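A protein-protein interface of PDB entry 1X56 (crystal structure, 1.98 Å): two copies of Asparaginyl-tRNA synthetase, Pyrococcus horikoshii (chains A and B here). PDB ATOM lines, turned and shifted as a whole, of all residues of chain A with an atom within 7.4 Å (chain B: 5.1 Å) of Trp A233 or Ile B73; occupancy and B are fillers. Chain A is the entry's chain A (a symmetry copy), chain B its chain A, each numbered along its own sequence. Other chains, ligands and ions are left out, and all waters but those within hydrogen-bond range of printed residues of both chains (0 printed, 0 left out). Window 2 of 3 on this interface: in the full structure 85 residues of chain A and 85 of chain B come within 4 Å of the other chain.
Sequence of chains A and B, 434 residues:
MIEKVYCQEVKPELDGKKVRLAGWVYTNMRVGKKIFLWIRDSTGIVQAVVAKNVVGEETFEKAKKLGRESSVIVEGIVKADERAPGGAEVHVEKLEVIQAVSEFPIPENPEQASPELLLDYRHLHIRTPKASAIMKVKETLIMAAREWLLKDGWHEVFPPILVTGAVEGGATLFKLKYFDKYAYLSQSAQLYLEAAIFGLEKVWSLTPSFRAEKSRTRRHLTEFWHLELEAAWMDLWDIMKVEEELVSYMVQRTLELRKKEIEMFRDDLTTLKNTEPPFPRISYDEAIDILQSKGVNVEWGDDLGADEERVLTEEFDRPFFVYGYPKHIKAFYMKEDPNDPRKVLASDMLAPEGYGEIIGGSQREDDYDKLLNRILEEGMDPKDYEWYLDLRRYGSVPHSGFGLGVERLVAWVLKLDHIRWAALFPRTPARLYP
Among the printed residues, pairs that only touch across the chains: Ile A197 with Trp B24 (3.9 Å), Trp A233 with Ile B2 (3.8 Å), Trp A233 with Lys B4 (3.9 Å), Trp A233 with Ala B22 (3.4 Å), Trp A233 with Gly B23 (3.5 Å), Trp A233 with Trp B24 (3.8 Å), Trp A233 with Ile B73 (3.6 Å), Trp A233 with Ile B98 (3.6 Å), Gly A395 with Ser B71 (3.4 Å), Ser A396 with Ile B98 (3.3 Å), Val A397 with Trp B24 (3.7 Å) and Val A397 with Ser B71 (3.6 Å).
NZ of Lys B4 is in salt-bridge range of OE2 of Glu A201 (2.8 Å).
The backbone carbonyl oxygen of Ser A396 lies within hydrogen-bond range of the side-chain hydroxyl of Ser B71, at 2.7 Å.
The indole nitrogen (NE1) of Trp B24 sits at hydrogen-bond distance from the backbone carbonyl oxygen (O) of Gly A395, at 3.0 Å.
No position is printed for both chains.
Hydrophobic or aromatic side chains of chain A that line the printed part of chain B: Trp A233 and Val A397.
Among the printed residues, 15 pairs touch across the chains.
OE2 of Glu A201 sits at hydrogen-bond distance from NE1 of Trp A233, 2.8 Å away.
O of Ile B73 sits at hydrogen-bond distance from N of Glu B96, at 2.9 Å.
N of Ile B98 lies within hydrogen-bond range of O of Ser B71.
The backbone NH of Val B72 is in hydrogen-bond range of the backbone carbonyl oxygen of Gly B23.
A ring nitrogen (ND1) of His A399 sits at hydrogen-bond distance from the backbone carbonyl oxygen of Val A397.
O of Pro A398 lies within hydrogen-bond range of N of Trp A233 (2.7 Å).
Of chain B, only Ile B2 (3.8 Å), Lys B4 (3.9 Å), Ala B22 (3.4 Å), Gly B23 (3.5 Å), Trp B24 (3.8 Å), Ile B73 (3.6 Å) and Ile B98 (3.6 Å) come within 4 Å of Trp A233.
Ile B73 touches one residue of chain A.
Of the printed residues of chain B, Val A397 touches Trp B24 (3.7 Å) and Ser B71 (3.6 Å).
Printed residues of chain A within 4 Å of Ala B22: Trp A233 (3.4 Å).
Printed residues of chain A within 4 Å of Lys B4: Glu A201 and Trp A233.
Of the printed residues of chain A, Ser B71 touches Gly A395 (3.4 Å), Ser A396 (2.7 Å) and Val A397 (3.6 Å).
Ala A232 touches none of the printed residues of chain B.
The nearest residue of chain B that does not touch Trp A233 is Val B72 (4.3 Å).
The nearest printed residue of chain A that does not touch Ser B71 is Trp A233 (5.1 Å).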
ATOM      1  N   ILE A 197      -3.897   2.673  12.270  1.00  0.00           N
ATOM      2  CA  ILE A 197      -4.630   1.432  11.918  1.00  0.00           C
ATOM      3  C   ILE A 197      -5.868   1.755  11.083  1.00  0.00           C
ATOM      4  O   ILE A 197      -6.352   0.911  10.345  1.00  0.00           O
ATOM      5  CB  ILE A 197      -5.071   0.574  13.150  1.00  0.00           C
ATOM      6  CG1 ILE A 197      -6.073   1.357  14.039  1.00  0.00           C
ATOM      7  CG2 ILE A 197      -3.858  -0.011  13.904  1.00  0.00           C
ATOM      8  CD1 ILE A 197      -6.702   0.567  15.172  1.00  0.00           C
ATOM      9  N   GLU A 201      -4.621  -0.805   8.943  1.00  0.00           N
ATOM     10  CA  GLU A 201      -5.203  -1.930   9.689  1.00  0.00           C
ATOM     11  C   GLU A 201      -4.237  -2.659  10.623  1.00  0.00           C
ATOM     12  O   GLU A 201      -4.561  -2.859  11.784  1.00  0.00           O
ATOM     13  CB  GLU A 201      -5.932  -2.915   8.759  1.00  0.00           C
ATOM     14  CG  GLU A 201      -7.193  -2.366   8.094  1.00  0.00           C
ATOM     15  CD  GLU A 201      -7.878  -3.467   7.295  1.00  0.00           C
ATOM     16  OE1 GLU A 201      -7.634  -3.523   6.050  1.00  0.00           O
ATOM     17  OE2 GLU A 201      -8.613  -4.285   7.936  1.00  0.00           O
ATOM     18  N   LYS A 202      -3.066  -3.050  10.135  1.00  0.00           N
ATOM     19  CA  LYS A 202      -2.091  -3.778  10.966  1.00  0.00           C
ATOM     20  C   LYS A 202      -0.798  -3.026  10.793  1.00  0.00           C
ATOM     21  O   LYS A 202      -0.267  -2.974   9.687  1.00  0.00           O
ATOM     22  CB  LYS A 202      -1.943  -5.217  10.497  1.00  0.00           C
ATOM     23  CG  LYS A 202      -3.206  -6.058  10.812  1.00  0.00           C
ATOM     24  CD  LYS A 202      -3.233  -7.384  10.051  1.00  0.00           C
ATOM     25  CE  LYS A 202      -2.131  -8.273  10.436  1.00  0.00           C
ATOM     26  NZ  LYS A 202      -2.230  -9.660   9.917  1.00  0.00           N
ATOM     27  N   ALA A 231      -3.409  -3.278  15.894  1.00  0.00           N
ATOM     28  CA  ALA A 231      -4.253  -3.914  14.854  1.00  0.00           C
ATOM     29  C   ALA A 231      -5.730  -3.605  15.093  1.00  0.00           C
ATOM     30  O   ALA A 231      -6.241  -3.854  16.190  1.00  0.00           O
ATOM     31  CB  ALA A 231      -4.050  -5.451  14.836  1.00  0.00           C
ATOM     32  N   ALA A 232      -6.374  -3.041  14.068  1.00  0.00           N
ATOM     33  CA  ALA A 232      -7.840  -2.971  13.938  1.00  0.00           C
ATOM     34  C   ALA A 232      -8.404  -4.366  14.069  1.00  0.00           C
ATOM     35  O   ALA A 232      -7.717  -5.348  13.679  1.00  0.00           O
ATOM     36  CB  ALA A 232      -8.239  -2.389  12.552  1.00  0.00           C
ATOM     37  N   TRP A 233      -9.639  -4.462  14.607  1.00  0.00           N
ATOM     38  CA  TRP A 233     -10.463  -5.697  14.615  1.00  0.00           C
ATOM     39  C   TRP A 233     -10.023  -6.725  15.648  1.00  0.00           C
ATOM     40  O   TRP A 233     -10.788  -7.642  15.923  1.00  0.00           O
ATOM     41  CB  TRP A 233     -10.589  -6.412  13.236  1.00  0.00           C
ATOM     42  CG  TRP A 233     -10.711  -5.475  12.072  1.00  0.00           C
ATOM     43  CD1 TRP A 233      -9.802  -5.299  11.052  1.00  0.00           C
ATOM     44  CD2 TRP A 233     -11.789  -4.567  11.813  1.00  0.00           C
ATOM     45  NE1 TRP A 233     -10.255  -4.339  10.171  1.00  0.00           N
ATOM     46  CE2 TRP A 233     -11.457  -3.847  10.622  1.00  0.00           C
ATOM     47  CE3 TRP A 233     -13.007  -4.275  12.468  1.00  0.00           C
ATOM     48  CZ2 TRP A 233     -12.301  -2.874  10.059  1.00  0.00           C
ATOM     49  CZ3 TRP A 233     -13.859  -3.288  11.911  1.00  0.00           C
ATOM     50  CH2 TRP A 233     -13.492  -2.604  10.708  1.00  0.00           C
ATOM     51  N   MET A 234      -8.839  -6.576  16.240  1.00  0.00           N
ATOM     52  CA  MET A 234      -8.314  -7.596  17.156  1.00  0.00           C
ATOM     53  C   MET A 234      -8.688  -7.303  18.586  1.00  0.00           C
ATOM     54  O   MET A 234      -8.526  -6.176  19.028  1.00  0.00           O
ATOM     55  CB  MET A 234      -6.790  -7.616  17.060  1.00  0.00           C
ATOM     56  CG  MET A 234      -6.312  -8.258  15.794  1.00  0.00           C
ATOM     57  SD  MET A 234      -4.646  -8.983  15.958  1.00  0.00           S
ATOM     58  CE  MET A 234      -4.291  -9.207  14.209  1.00  0.00           C
ATOM     59  N   ASP A 235      -9.137  -8.312  19.329  1.00  0.00           N
ATOM     60  CA  ASP A 235      -9.359  -8.143  20.782  1.00  0.00           C
ATOM     61  C   ASP A 235      -8.137  -8.630  21.569  1.00  0.00           C
ATOM     62  O   ASP A 235      -7.106  -8.972  20.984  1.00  0.00           O
ATOM     63  CB  ASP A 235     -10.607  -8.871  21.272  1.00  0.00           C
ATOM     64  CG  ASP A 235     -10.537 -10.380  21.092  1.00  0.00           C
ATOM     65  OD1 ASP A 235      -9.442 -11.012  20.939  1.00  0.00           O
ATOM     66  OD2 ASP A 235     -11.590 -11.046  21.051  1.00  0.00           O
ATOM     67  N   ASP A 238      -6.826 -12.177  20.621  1.00  0.00           N
ATOM     68  CA  ASP A 238      -6.200 -12.131  19.303  1.00  0.00           C
ATOM     69  C   ASP A 238      -4.790 -11.560  19.422  1.00  0.00           C
ATOM     70  O   ASP A 238      -3.867 -12.113  18.858  1.00  0.00           O
ATOM     71  CB  ASP A 238      -6.947 -11.178  18.394  1.00  0.00           C
ATOM     72  CG  ASP A 238      -8.332 -11.666  18.033  1.00  0.00           C
ATOM     73  OD1 ASP A 238      -9.143 -10.805  17.683  1.00  0.00           O
ATOM     74  OD2 ASP A 238      -8.676 -12.867  18.067  1.00  0.00           O
ATOM     75  N   GLN A 363      -6.215  -4.649  24.999  1.00  0.00           N
ATOM     76  CA  GLN A 363      -7.270  -4.157  24.115  1.00  0.00           C
ATOM     77  C   GLN A 363      -7.517  -2.707  24.519  1.00  0.00           C
ATOM     78  O   GLN A 363      -7.428  -2.350  25.719  1.00  0.00           O
ATOM     79  CB  GLN A 363      -8.549  -5.032  24.177  1.00  0.00           C
ATOM     80  CG  GLN A 363      -9.636  -4.638  23.132  1.00  0.00           C
ATOM     81  CD  GLN A 363     -10.687  -5.693  22.973  1.00  0.00           C
ATOM     82  OE1 GLN A 363     -10.608  -6.742  23.609  1.00  0.00           O
ATOM     83  NE2 GLN A 363     -11.697  -5.423  22.150  1.00  0.00           N
ATOM     84  N   GLY A 395     -15.592   6.557  13.193  1.00  0.00           N
ATOM     85  CA  GLY A 395     -15.530   5.199  12.677  1.00  0.00           C
ATOM     86  C   GLY A 395     -14.628   4.338  13.558  1.00  0.00           C
ATOM     87  O   GLY A 395     -13.805   3.546  13.058  1.00  0.00           O
ATOM     88  N   SER A 396     -14.809   4.492  14.869  1.00  0.00           N
ATOM     89  CA  SER A 396     -14.196   3.637  15.882  1.00  0.00           C
ATOM     90  C   SER A 396     -14.321   2.167  15.501  1.00  0.00           C
ATOM     91  O   SER A 396     -15.348   1.718  14.936  1.00  0.00           O
ATOM     92  CB  SER A 396     -14.882   3.815  17.238  1.00  0.00           C
ATOM     93  OG  SER A 396     -14.074   3.248  18.288  1.00  0.00           O
ATOM     94  N   VAL A 397     -13.279   1.394  15.810  1.00  0.00           N
ATOM     95  CA  VAL A 397     -13.349  -0.057  15.603  1.00  0.00           C
ATOM     96  C   VAL A 397     -12.697  -0.679  16.838  1.00  0.00           C
ATOM     97  O   VAL A 397     -11.847  -0.043  17.457  1.00  0.00           O
ATOM     98  CB  VAL A 397     -12.632  -0.516  14.267  1.00  0.00           C
ATOM     99  CG1 VAL A 397     -13.397   0.015  13.022  1.00  0.00           C
ATOM    100  CG2 VAL A 397     -11.062  -0.143  14.247  1.00  0.00           C
ATOM    101  N   PRO A 398     -13.065  -1.889  17.223  1.00  0.00           N
ATOM    102  CA  PRO A 398     -12.281  -2.557  18.282  1.00  0.00           C
ATOM    103  C   PRO A 398     -10.823  -2.742  17.794  1.00  0.00           C
ATOM    104  O   PRO A 398     -10.596  -2.929  16.573  1.00  0.00           O
ATOM    105  CB  PRO A 398     -12.951  -3.920  18.455  1.00  0.00           C
ATOM    106  CG  PRO A 398     -14.040  -4.019  17.381  1.00  0.00           C
ATOM    107  CD  PRO A 398     -14.173  -2.708  16.693  1.00  0.00           C
ATOM    108  N   HIS A 399      -9.872  -2.647  18.714  1.00  0.00           N
ATOM    109  CA  HIS A 399      -8.462  -2.768  18.384  1.00  0.00           C
ATOM    110  C   HIS A 399      -7.603  -2.978  19.631  1.00  0.00           C
ATOM    111  O   HIS A 399      -8.038  -2.672  20.744  1.00  0.00           O
ATOM    112  CB  HIS A 399      -7.950  -1.582  17.513  1.00  0.00           C
ATOM    113  CG  HIS A 399      -7.944  -0.249  18.213  1.00  0.00           C
ATOM    114  ND1 HIS A 399      -9.075   0.540  18.349  1.00  0.00           N
ATOM    115  CD2 HIS A 399      -6.931   0.455  18.777  1.00  0.00           C
ATOM    116  CE1 HIS A 399      -8.762   1.663  18.981  1.00  0.00           C
ATOM    117  NE2 HIS A 399      -7.463   1.640  19.248  1.00  0.00           N
ATOM    118  N   SER A 400      -6.414  -3.558  19.428  1.00  0.00           N
ATOM    119  CA  SER A 400      -5.500  -3.954  20.495  1.00  0.00           C
ATOM    120  C   SER A 400      -4.085  -3.824  19.985  1.00  0.00           C
ATOM    121  O   SER A 400      -3.826  -3.828  18.759  1.00  0.00           O
ATOM    122  CB  SER A 400      -5.689  -5.431  20.841  1.00  0.00           C
ATOM    123  OG  SER A 400      -7.017  -5.725  21.167  1.00  0.00           O
ATOM    124  N   ILE B   2     -12.508 -11.299  14.387  1.00  0.00           N
ATOM    125  CA  ILE B   2     -13.215 -10.923  13.148  1.00  0.00           C
ATOM    126  C   ILE B   2     -12.412 -11.582  12.013  1.00  0.00           C
ATOM    127  O   ILE B   2     -11.240 -11.213  11.804  1.00  0.00           O
ATOM    128  CB  ILE B   2     -13.307  -9.333  13.025  1.00  0.00           C
ATOM    129  CG1 ILE B   2     -14.474  -8.789  13.880  1.00  0.00           C
ATOM    130  CG2 ILE B   2     -13.395  -8.842  11.553  1.00  0.00           C
ATOM    131  CD1 ILE B   2     -14.433  -7.279  14.224  1.00  0.00           C
ATOM    132  N   LYS B   4     -11.843 -11.709   8.418  1.00  0.00           N
ATOM    133  CA  LYS B   4     -12.321 -10.812   7.359  1.00  0.00           C
ATOM    134  C   LYS B   4     -11.719 -11.198   6.024  1.00  0.00           C
ATOM    135  O   LYS B   4     -10.706 -11.880   5.972  1.00  0.00           O
ATOM    136  CB  LYS B   4     -12.043  -9.353   7.724  1.00  0.00           C
ATOM    137  CG  LYS B   4     -10.531  -8.978   7.865  1.00  0.00           C
ATOM    138  CD  LYS B   4     -10.322  -7.470   7.817  1.00  0.00           C
ATOM    139  CE  LYS B   4     -10.552  -6.985   6.362  1.00  0.00           C
ATOM    140  NZ  LYS B   4     -10.397  -5.546   6.162  1.00  0.00           N
ATOM    141  N   ARG B  20     -16.912 -11.828   4.406  1.00  0.00           N
ATOM    142  CA  ARG B  20     -17.129 -10.836   5.438  1.00  0.00           C
ATOM    143  C   ARG B  20     -16.135  -9.718   5.245  1.00  0.00           C
ATOM    144  O   ARG B  20     -14.927  -9.920   5.421  1.00  0.00           O
ATOM    145  CB  ARG B  20     -16.863 -11.494   6.784  1.00  0.00           C
ATOM    146  CG  ARG B  20     -17.115 -10.664   8.001  1.00  0.00           C
ATOM    147  CD  ARG B  20     -16.961 -11.622   9.180  1.00  0.00           C
ATOM    148  NE  ARG B  20     -17.807 -11.335  10.307  1.00  0.00           N
ATOM    149  CZ  ARG B  20     -17.394 -10.591  11.321  1.00  0.00           C
ATOM    150  NH1 ARG B  20     -16.162 -10.087  11.260  1.00  0.00           N
ATOM    151  NH2 ARG B  20     -18.193 -10.340  12.374  1.00  0.00           N
ATOM    152  N   LEU B  21     -16.642  -8.532   4.936  1.00  0.00           N
ATOM    153  CA  LEU B  21     -15.814  -7.318   4.825  1.00  0.00           C
ATOM    154  C   LEU B  21     -15.794  -6.578   6.146  1.00  0.00           C
ATOM    155  O   LEU B  21     -16.752  -6.643   6.912  1.00  0.00           O
ATOM    156  CB  LEU B  21     -16.376  -6.402   3.739  1.00  0.00           C
ATOM    157  CG  LEU B  21     -16.629  -6.939   2.317  1.00  0.00           C
ATOM    158  CD1 LEU B  21     -17.085  -5.736   1.462  1.00  0.00           C
ATOM    159  CD2 LEU B  21     -15.397  -7.680   1.691  1.00  0.00           C
ATOM    160  N   ALA B  22     -14.683  -5.927   6.454  1.00  0.00           N
ATOM    161  CA  ALA B  22     -14.600  -5.100   7.671  1.00  0.00           C
ATOM    162  C   ALA B  22     -13.857  -3.868   7.235  1.00  0.00           C
ATOM    163  O   ALA B  22     -12.721  -3.942   6.728  1.00  0.00           O
ATOM    164  CB  ALA B  22     -13.848  -5.874   8.846  1.00  0.00           C
ATOM    165  N   GLY B  23     -14.504  -2.715   7.358  1.00  0.00           N
ATOM    166  CA  GLY B  23     -13.848  -1.514   6.916  1.00  0.00           C
ATOM    167  C   GLY B  23     -14.667  -0.274   7.145  1.00  0.00           C
ATOM    168  O   GLY B  23     -15.458  -0.205   8.104  1.00  0.00           O
ATOM    169  N   TRP B  24     -14.430   0.722   6.292  1.00  0.00           N
ATOM    170  CA  TRP B  24     -14.985   2.038   6.483  1.00  0.00           C
ATOM    171  C   TRP B  24     -15.707   2.497   5.205  1.00  0.00           C
ATOM    172  O   TRP B  24     -15.213   2.261   4.091  1.00  0.00           O
ATOM    173  CB  TRP B  24     -13.869   3.033   6.824  1.00  0.00           C
ATOM    174  CG  TRP B  24     -13.227   2.713   8.158  1.00  0.00           C
ATOM    175  CD1 TRP B  24     -13.610   3.195   9.370  1.00  0.00           C
ATOM    176  CD2 TRP B  24     -12.143   1.811   8.402  1.00  0.00           C
ATOM    177  NE1 TRP B  24     -12.841   2.642  10.365  1.00  0.00           N
ATOM    178  CE2 TRP B  24     -11.922   1.795   9.802  1.00  0.00           C
ATOM    179  CE3 TRP B  24     -11.328   1.001   7.579  1.00  0.00           C
ATOM    180  CZ2 TRP B  24     -10.909   1.015  10.407  1.00  0.00           C
ATOM    181  CZ3 TRP B  24     -10.343   0.195   8.177  1.00  0.00           C
ATOM    182  CH2 TRP B  24     -10.130   0.229   9.580  1.00  0.00           C
ATOM    183  N   SER B  71     -17.786   3.005  10.280  1.00  0.00           N
ATOM    184  CA  SER B  71     -17.162   1.668  10.390  1.00  0.00           C
ATOM    185  C   SER B  71     -18.223   0.605  10.346  1.00  0.00           C
ATOM    186  O   SER B  71     -19.234   0.686  11.066  1.00  0.00           O
ATOM    187  CB  SER B  71     -16.305   1.550  11.646  1.00  0.00           C
ATOM    188  OG  SER B  71     -16.994   2.024  12.808  1.00  0.00           O
ATOM    189  N   VAL B  72     -18.009  -0.390   9.495  1.00  0.00           N
ATOM    190  CA  VAL B  72     -19.006  -1.402   9.207  1.00  0.00           C
ATOM    191  C   VAL B  72     -18.391  -2.790   9.041  1.00  0.00           C
ATOM    192  O   VAL B  72     -17.213  -2.935   8.615  1.00  0.00           O
ATOM    193  CB  VAL B  72     -19.875  -1.046   7.943  1.00  0.00           C
ATOM    194  CG1 VAL B  72     -20.669   0.256   8.176  1.00  0.00           C
ATOM    195  CG2 VAL B  72     -19.000  -0.959   6.708  1.00  0.00           C
ATOM    196  N   ILE B  73     -19.171  -3.794   9.423  1.00  0.00           N
ATOM    197  CA  ILE B  73     -18.905  -5.189   9.056  1.00  0.00           C
ATOM    198  C   ILE B  73     -20.003  -5.564   8.071  1.00  0.00           C
ATOM    199  O   ILE B  73     -21.183  -5.304   8.327  1.00  0.00           O
ATOM    200  CB  ILE B  73     -18.981  -6.166  10.286  1.00  0.00           C
ATOM    201  CG1 ILE B  73     -18.060  -5.749  11.436  1.00  0.00           C
ATOM    202  CG2 ILE B  73     -18.769  -7.619   9.826  1.00  0.00           C
ATOM    203  CD1 ILE B  73     -16.742  -5.309  10.982  1.00  0.00           C
ATOM    204  N   VAL B  74     -19.620  -6.149   6.950  1.00  0.00           N
ATOM    205  CA  VAL B  74     -20.550  -6.511   5.907  1.00  0.00           C
ATOM    206  C   VAL B  74     -20.388  -8.005   5.569  1.00  0.00           C
ATOM    207  O   VAL B  74     -19.285  -8.452   5.221  1.00  0.00           O
ATOM    208  CB  VAL B  74     -20.300  -5.630   4.640  1.00  0.00           C
ATOM    209  CG1 VAL B  74     -21.084  -6.120   3.459  1.00  0.00           C
ATOM    210  CG2 VAL B  74     -20.672  -4.197   4.938  1.00  0.00           C
ATOM    211  N   GLU B  75     -21.474  -8.768   5.645  1.00  0.00           N
ATOM    212  CA  GLU B  75     -21.440 -10.127   5.117  1.00  0.00           C
ATOM    213  C   GLU B  75     -22.346 -10.278   3.918  1.00  0.00           C
ATOM    214  O   GLU B  75     -23.467  -9.769   3.895  1.00  0.00           O
ATOM    215  CB  GLU B  75     -21.843 -11.130   6.181  1.00  0.00           C
ATOM    216  CG  GLU B  75     -20.966 -11.053   7.419  1.00  0.00           C
ATOM    217  CD  GLU B  75     -21.339 -12.132   8.440  1.00  0.00           C
ATOM    218  OE1 GLU B  75     -20.494 -12.433   9.312  1.00  0.00           O
ATOM    219  OE2 GLU B  75     -22.473 -12.694   8.354  1.00  0.00           O
ATOM    220  N   LYS B  94     -25.993  -9.210   5.537  1.00  0.00           N
ATOM    221  CA  LYS B  94     -25.990  -8.679   6.859  1.00  0.00           C
ATOM    222  C   LYS B  94     -25.104  -7.441   6.885  1.00  0.00           C
ATOM    223  O   LYS B  94     -23.999  -7.474   6.356  1.00  0.00           O
ATOM    224  CB  LYS B  94     -25.498  -9.757   7.830  1.00  0.00           C
ATOM    225  CG  LYS B  94     -25.452  -9.345   9.277  1.00  0.00           C
ATOM    226  CD  LYS B  94     -24.521 -10.291  10.117  1.00  0.00           C
ATOM    227  CE  LYS B  94     -24.580  -9.960  11.645  1.00  0.00           C
ATOM    228  NZ  LYS B  94     -24.579  -8.460  11.969  1.00  0.00           N
ATOM    229  N   LEU B  95     -25.593  -6.368   7.513  1.00  0.00           N
ATOM    230  CA  LEU B  95     -24.849  -5.134   7.685  1.00  0.00           C
ATOM    231  C   LEU B  95     -24.802  -4.787   9.158  1.00  0.00           C
ATOM    232  O   LEU B  95     -25.833  -4.557   9.761  1.00  0.00           O
ATOM    233  CB  LEU B  95     -25.519  -3.968   6.930  1.00  0.00           C
ATOM    234  CG  LEU B  95     -24.949  -2.547   7.127  1.00  0.00           C
ATOM    235  CD1 LEU B  95     -23.500  -2.403   6.569  1.00  0.00           C
ATOM    236  CD2 LEU B  95     -25.883  -1.523   6.498  1.00  0.00           C
ATOM    237  N   GLU B  96     -23.617  -4.750   9.746  1.00  0.00           N
ATOM    238  CA  GLU B  96     -23.468  -4.406  11.146  1.00  0.00           C
ATOM    239  C   GLU B  96     -22.768  -3.073  11.185  1.00  0.00           C
ATOM    240  O   GLU B  96     -21.637  -2.940  10.694  1.00  0.00           O
ATOM    241  CB  GLU B  96     -22.635  -5.476  11.834  1.00  0.00           C
ATOM    242  CG  GLU B  96     -22.362  -5.300  13.305  1.00  0.00           C
ATOM    243  CD  GLU B  96     -21.511  -6.486  13.827  1.00  0.00           C
ATOM    244  OE1 GLU B  96     -20.868  -6.340  14.927  1.00  0.00           O
ATOM    245  OE2 GLU B  96     -21.462  -7.567  13.119  1.00  0.00           O
ATOM    246  N   ILE B  98     -20.862  -0.420  13.071  1.00  0.00           N
ATOM    247  CA  ILE B  98     -20.117  -0.253  14.299  1.00  0.00           C
ATOM    248  C   ILE B  98     -20.258   1.194  14.784  1.00  0.00           C
ATOM    249  O   ILE B  98     -20.609   1.433  15.952  1.00  0.00           O
ATOM    250  CB  ILE B  98     -18.623  -0.653  14.112  1.00  0.00           C
ATOM    251  CG1 ILE B  98     -18.527  -2.104  13.668  1.00  0.00           C
ATOM    252  CG2 ILE B  98     -17.816  -0.388  15.404  1.00  0.00           C
ATOM    253  CD1 ILE B  98     -17.105  -2.503  13.331  1.00  0.00           C
